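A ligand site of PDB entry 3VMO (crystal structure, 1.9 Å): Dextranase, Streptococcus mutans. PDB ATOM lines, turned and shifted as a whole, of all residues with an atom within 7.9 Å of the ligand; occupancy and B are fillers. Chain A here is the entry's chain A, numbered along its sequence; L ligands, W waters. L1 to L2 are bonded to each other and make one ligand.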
ATOM      1  N   GLN A  38      20.952 -30.050  22.254  1.00  0.00           N
ATOM      2  CA  GLN A  38      22.111 -30.266  23.069  1.00  0.00           C
ATOM      3  C   GLN A  38      21.981 -29.477  24.365  1.00  0.00           C
ATOM      4  O   GLN A  38      21.082 -28.644  24.501  1.00  0.00           O
ATOM      5  CB  GLN A  38      23.368 -29.792  22.348  1.00  0.00           C
ATOM      6  CG  GLN A  38      23.348 -28.303  21.933  1.00  0.00           C
ATOM      7  CD  GLN A  38      24.574 -27.911  21.171  1.00  0.00           C
ATOM      8  OE1 GLN A  38      25.696 -28.161  21.612  1.00  0.00           O
ATOM      9  NE2 GLN A  38      24.380 -27.314  20.031  1.00  0.00           N
ATOM     10  N   ASN A  39      22.871 -29.779  25.317  1.00  0.00           N
ATOM     11  CA  ASN A  39      23.020 -28.957  26.521  1.00  0.00           C
ATOM     12  C   ASN A  39      23.584 -27.602  26.208  1.00  0.00           C
ATOM     13  O   ASN A  39      24.576 -27.467  25.472  1.00  0.00           O
ATOM     14  CB  ASN A  39      23.865 -29.682  27.546  1.00  0.00           C
ATOM     15  CG  ASN A  39      23.065 -30.798  28.251  1.00  0.00           C
ATOM     16  OD1 ASN A  39      21.950 -30.573  28.744  1.00  0.00           O
ATOM     17  ND2 ASN A  39      23.610 -31.983  28.294  1.00  0.00           N
ATOM     18  N   ILE A  40      22.917 -26.599  26.738  1.00  0.00           N
ATOM     19  CA  ILE A  40      23.340 -25.210  26.605  1.00  0.00           C
ATOM     20  C   ILE A  40      23.671 -24.735  28.026  1.00  0.00           C
ATOM     21  O   ILE A  40      22.895 -24.974  28.982  1.00  0.00           O
ATOM     22  CB  ILE A  40      22.251 -24.336  25.967  1.00  0.00           C
ATOM     23  CG1 ILE A  40      21.915 -24.806  24.522  1.00  0.00           C
ATOM     24  CG2 ILE A  40      22.724 -22.860  25.881  1.00  0.00           C
ATOM     25  CD1 ILE A  40      23.039 -24.696  23.559  1.00  0.00           C
ATOM     26  N   THR A  41      24.849 -24.134  28.186  1.00  0.00           N
ATOM     27  CA  THR A  41      25.346 -23.726  29.509  1.00  0.00           C
ATOM     28  C   THR A  41      25.467 -22.173  29.590  1.00  0.00           C
ATOM     29  O   THR A  41      26.098 -21.526  28.734  1.00  0.00           O
ATOM     30  CB  THR A  41      26.718 -24.339  29.788  1.00  0.00           C
ATOM     31  OG1 THR A  41      26.620 -25.785  29.857  1.00  0.00           O
ATOM     32  CG2 THR A  41      27.314 -23.797  31.137  1.00  0.00           C
ATOM     33  N   GLN A  57      26.833 -21.017  37.372  1.00  0.00           N
ATOM     34  CA  GLN A  57      26.494 -21.670  36.085  1.00  0.00           C
ATOM     35  C   GLN A  57      25.191 -22.379  36.106  1.00  0.00           C
ATOM     36  O   GLN A  57      24.709 -22.775  37.177  1.00  0.00           O
ATOM     37  CB  GLN A  57      27.587 -22.617  35.664  1.00  0.00           C
ATOM     38  CG  GLN A  57      27.420 -24.034  36.208  1.00  0.00           C
ATOM     39  CD  GLN A  57      27.354 -25.051  35.068  1.00  0.00           C
ATOM     40  OE1 GLN A  57      26.261 -25.521  34.634  1.00  0.00           O
ATOM     41  NE2 GLN A  57      28.544 -25.390  34.566  1.00  0.00           N
ATOM     42  N   TYR A  58      24.615 -22.609  34.926  1.00  0.00           N
ATOM     43  CA  TYR A  58      23.367 -23.318  34.838  1.00  0.00           C
ATOM     44  C   TYR A  58      23.280 -23.974  33.435  1.00  0.00           C
ATOM     45  O   TYR A  58      23.664 -23.349  32.458  1.00  0.00           O
ATOM     46  CB  TYR A  58      22.248 -22.324  34.993  1.00  0.00           C
ATOM     47  CG  TYR A  58      20.923 -23.000  34.919  1.00  0.00           C
ATOM     48  CD1 TYR A  58      20.320 -23.516  36.062  1.00  0.00           C
ATOM     49  CD2 TYR A  58      20.276 -23.148  33.690  1.00  0.00           C
ATOM     50  CE1 TYR A  58      19.096 -24.160  35.983  1.00  0.00           C
ATOM     51  CE2 TYR A  58      19.047 -23.801  33.602  1.00  0.00           C
ATOM     52  CZ  TYR A  58      18.459 -24.299  34.749  1.00  0.00           C
ATOM     53  OH  TYR A  58      17.245 -24.934  34.666  1.00  0.00           O
ATOM     54  N   THR A  59      22.854 -25.236  33.371  1.00  0.00           N
ATOM     55  CA  THR A  59      22.909 -26.012  32.097  1.00  0.00           C
ATOM     56  C   THR A  59      21.557 -26.635  31.891  1.00  0.00           C
ATOM     57  O   THR A  59      20.978 -27.222  32.809  1.00  0.00           O
ATOM     58  CB  THR A  59      23.993 -27.092  32.122  1.00  0.00           C
ATOM     59  OG1 THR A  59      25.277 -26.492  32.218  1.00  0.00           O
ATOM     60  CG2 THR A  59      23.992 -27.991  30.850  1.00  0.00           C
ATOM     61  N   LYS A  60      21.017 -26.458  30.680  1.00  0.00           N
ATOM     62  CA  LYS A  60      19.784 -27.111  30.324  1.00  0.00           C
ATOM     63  C   LYS A  60      19.857 -27.694  28.905  1.00  0.00           C
ATOM     64  O   LYS A  60      20.346 -27.062  27.998  1.00  0.00           O
ATOM     65  CB  LYS A  60      18.606 -26.170  30.438  1.00  0.00           C
ATOM     66  CG  LYS A  60      17.270 -26.944  30.477  1.00  0.00           C
ATOM     67  CD  LYS A  60      16.128 -26.014  30.794  1.00  0.00           C
ATOM     68  CE  LYS A  60      14.789 -26.572  30.356  1.00  0.00           C
ATOM     69  NZ  LYS A  60      14.536 -27.894  31.031  1.00  0.00           N
ATOM     70  N   TYR A  61      19.325 -28.904  28.758  1.00  0.00           N
ATOM     71  CA  TYR A  61      19.162 -29.545  27.451  1.00  0.00           C
ATOM     72  C   TYR A  61      18.012 -28.910  26.685  1.00  0.00           C
ATOM     73  O   TYR A  61      16.886 -28.841  27.164  1.00  0.00           O
ATOM     74  CB  TYR A  61      18.990 -31.061  27.643  1.00  0.00           C
ATOM     75  CG  TYR A  61      18.894 -31.860  26.352  1.00  0.00           C
ATOM     76  CD1 TYR A  61      17.656 -32.082  25.732  1.00  0.00           C
ATOM     77  CD2 TYR A  61      20.031 -32.411  25.777  1.00  0.00           C
ATOM     78  CE1 TYR A  61      17.576 -32.837  24.528  1.00  0.00           C
ATOM     79  CE2 TYR A  61      19.956 -33.163  24.590  1.00  0.00           C
ATOM     80  CZ  TYR A  61      18.730 -33.361  23.981  1.00  0.00           C
ATOM     81  OH  TYR A  61      18.665 -34.109  22.826  1.00  0.00           O
ATOM     82  N   LEU A  62      18.310 -28.417  25.501  1.00  0.00           N
ATOM     83  CA  LEU A  62      17.390 -27.656  24.691  1.00  0.00           C
ATOM     84  C   LEU A  62      17.393 -28.206  23.259  1.00  0.00           C
ATOM     85  O   LEU A  62      18.450 -28.505  22.702  1.00  0.00           O
ATOM     86  CB  LEU A  62      17.792 -26.173  24.650  1.00  0.00           C
ATOM     87  CG  LEU A  62      17.639 -25.410  25.974  1.00  0.00           C
ATOM     88  CD1 LEU A  62      18.219 -23.982  25.860  1.00  0.00           C
ATOM     89  CD2 LEU A  62      16.147 -25.344  26.385  1.00  0.00           C
ATOM     90  N   SER A  95      27.266 -21.030  26.211  1.00  0.00           N
ATOM     91  CA  SER A  95      28.080 -21.889  25.367  1.00  0.00           C
ATOM     92  C   SER A  95      27.295 -23.141  24.993  1.00  0.00           C
ATOM     93  O   SER A  95      26.374 -23.515  25.694  1.00  0.00           O
ATOM     94  CB  SER A  95      29.418 -22.251  26.033  1.00  0.00           C
ATOM     95  OG  SER A  95      29.242 -22.775  27.335  1.00  0.00           O
ATOM     96  N   ASP A  96      27.673 -23.782  23.888  1.00  0.00           N
ATOM     97  CA  ASP A  96      27.036 -25.035  23.523  1.00  0.00           C
ATOM     98  C   ASP A  96      27.770 -26.219  24.170  1.00  0.00           C
ATOM     99  O   ASP A  96      28.747 -26.049  24.976  1.00  0.00           O
ATOM    100  CB  ASP A  96      26.980 -25.168  21.979  1.00  0.00           C
ATOM    101  CG  ASP A  96      28.356 -25.244  21.325  1.00  0.00           C
ATOM    102  OD1 ASP A  96      29.374 -25.566  21.984  1.00  0.00           O
ATOM    103  OD2 ASP A  96      28.452 -24.982  20.111  1.00  0.00           O
ATOM    104  N   SER A  97      27.391 -27.448  23.789  1.00  0.00           N
ATOM    105  CA  SER A  97      27.991 -28.576  24.440  1.00  0.00           C
ATOM    106  C   SER A  97      29.441 -28.823  23.961  1.00  0.00           C
ATOM    107  O   SER A  97      30.170 -29.602  24.572  1.00  0.00           O
ATOM    108  CB  SER A  97      27.094 -29.808  24.307  1.00  0.00           C
ATOM    109  OG  SER A  97      27.065 -30.244  22.956  1.00  0.00           O
ATOM    110  N   GLN A  98      29.868 -28.140  22.902  1.00  0.00           N
ATOM    111  CA  GLN A  98      31.279 -28.209  22.511  1.00  0.00           C
ATOM    112  C   GLN A  98      32.101 -26.999  23.042  1.00  0.00           C
ATOM    113  O   GLN A  98      33.245 -26.770  22.606  1.00  0.00           O
ATOM    114  CB  GLN A  98      31.453 -28.381  20.985  1.00  0.00           C
ATOM    115  CG  GLN A  98      30.842 -29.689  20.412  1.00  0.00           C
ATOM    116  CD  GLN A  98      31.582 -30.938  20.882  1.00  0.00           C
ATOM    117  OE1 GLN A  98      31.057 -31.736  21.693  1.00  0.00           O
ATOM    118  NE2 GLN A  98      32.803 -31.138  20.377  1.00  0.00           N
ATOM    119  N   ASN A  99      31.527 -26.237  23.987  1.00  0.00           N
ATOM    120  CA  ASN A  99      32.157 -25.013  24.534  1.00  0.00           C
ATOM    121  C   ASN A  99      32.351 -23.858  23.563  1.00  0.00           C
ATOM    122  O   ASN A  99      33.124 -22.955  23.843  1.00  0.00           O
ATOM    123  CB  ASN A  99      33.496 -25.331  25.232  1.00  0.00           C
ATOM    124  CG  ASN A  99      33.344 -26.330  26.359  1.00  0.00           C
ATOM    125  OD1 ASN A  99      32.397 -26.270  27.136  1.00  0.00           O
ATOM    126  ND2 ASN A  99      34.282 -27.260  26.454  1.00  0.00           N
HETATM  127  C1  LIG L   1      22.284 -30.593  34.016  1.00  0.00           C
HETATM  128  C2  LIG L   1      21.381 -30.636  32.762  1.00  0.00           C
HETATM  129  C3  LIG L   1      21.539 -31.968  31.988  1.00  0.00           C
HETATM  130  C4  LIG L   1      23.015 -32.250  31.700  1.00  0.00           C
HETATM  131  C5  LIG L   1      23.834 -32.144  32.996  1.00  0.00           C
HETATM  132  C6  LIG L   1      25.347 -32.283  32.782  1.00  0.00           C
HETATM  133  O1  LIG L   1      21.833 -31.473  35.033  1.00  0.00           O
HETATM  134  O2  LIG L   1      20.030 -30.342  33.126  1.00  0.00           O
HETATM  135  O3  LIG L   1      20.853 -31.914  30.759  1.00  0.00           O
HETATM  136  O4  LIG L   1      23.176 -33.487  31.046  1.00  0.00           O
HETATM  137  O5  LIG L   1      23.607 -30.881  33.600  1.00  0.00           O
HETATM  138  O6  LIG L   1      25.798 -31.281  31.871  1.00  0.00           O
HETATM  139  C1  LG2 L   2      27.121 -31.602  31.380  1.00  0.00           C
HETATM  140  C2  LG2 L   2      27.624 -30.503  30.429  1.00  0.00           C
HETATM  141  C3  LG2 L   2      26.986 -30.606  29.033  1.00  0.00           C
HETATM  142  C4  LG2 L   2      27.084 -32.023  28.452  1.00  0.00           C
HETATM  143  C5  LG2 L   2      26.654 -33.072  29.472  1.00  0.00           C
HETATM  144  C6  LG2 L   2      26.970 -34.471  28.936  1.00  0.00           C
HETATM  145  O1  LG2 L   2      27.347 -29.218  30.966  1.00  0.00           O
HETATM  146  O2  LG2 L   2      27.531 -29.656  28.105  1.00  0.00           O
HETATM  147  O3  LG2 L   2      26.264 -32.122  27.290  1.00  0.00           O
HETATM  148  O4  LG2 L   2      27.225 -32.888  30.775  1.00  0.00           O
HETATM  149  O5  LG2 L   2      26.586 -35.409  29.928  1.00  0.00           O
HETATM  150  O   HOH W   1      29.893 -30.280  27.082  1.00  0.00           O
HETATM  151  O   HOH W   2      25.036 -37.532  29.603  1.00  0.00           O
HETATM  152  O   HOH W   3      26.572 -27.246  27.603  1.00  0.00           O
HETATM  153  O   HOH W   4      29.158 -26.948  30.057  1.00  0.00           O
HETATM  154  O   HOH W   5      18.173 -30.106  31.218  1.00  0.00           O
HETATM  155  O   HOH W   6      24.657 -32.185  24.719  1.00  0.00           O
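The backbone carbonyl oxygen (O) of Thr 59 lies within hydrogen-bond range of an oxygen (O2) of LIG L1, at 3.3 Å. OD1 of Asn 39 is in hydrogen-bond range of O3 of LIG L1 (2.7 Å).
OD1 of Asn 39 lies within hydrogen-bond range of N of Tyr 61. OG1 of Thr 41 is in hydrogen-bond range of OG1 of Thr 59, 2.8 Å away. The backbone carbonyl oxygen (O) of Asn 39 sits at hydrogen-bond distance from the backbone NH (N) of Ser 97, at 3.3 Å. The side-chain hydroxyl (OG) of Ser 97 lies within hydrogen-bond range of the side-chain amide oxygen (OE1) of Gln 38, 2.8 Å away. O of Thr 41 lies within hydrogen-bond range of N of Ser 95, 2.8 Å away. The side-chain amide oxygen of Gln 57 sits at hydrogen-bond distance from the side-chain hydroxyl of Thr 59 (2.8 Å).
Thr 41 touches the ligand. CB of Tyr 61 touches O3 of LIG L1, 3.7 Å away. CB of Ser 97 touches O2 of LG2 L2 (3.8 Å). Five residues have an atom within 4 Å of the ligand: Asn 39, Thr 41, Thr 59, Tyr 61 and Ser 97. The nearest printed residue that does not touch the ligand is Lys 60 (4.3 Å).
Water W3 lies within hydrogen-bond range of O2 of LG2 L2, OG1 of Thr 41 and O of Asn 39. Water W1 lies within hydrogen-bond range of the backbone carbonyl oxygen of Ser 97 and an oxygen (O2) of LG2 L2. Water W5 lies within hydrogen-bond range of O2 of LIG L1 (2.7 Å) and N of Tyr 61 (3.0 Å). Water W6 lies within hydrogen-bond range of an oxygen (O3) of LG2 L2 and the backbone NH of Asn 39. Water W4 lies within hydrogen-bond range of OG1 of Thr 41 (2.8 Å) and O1 of LG2 L2 (3.0 Å).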
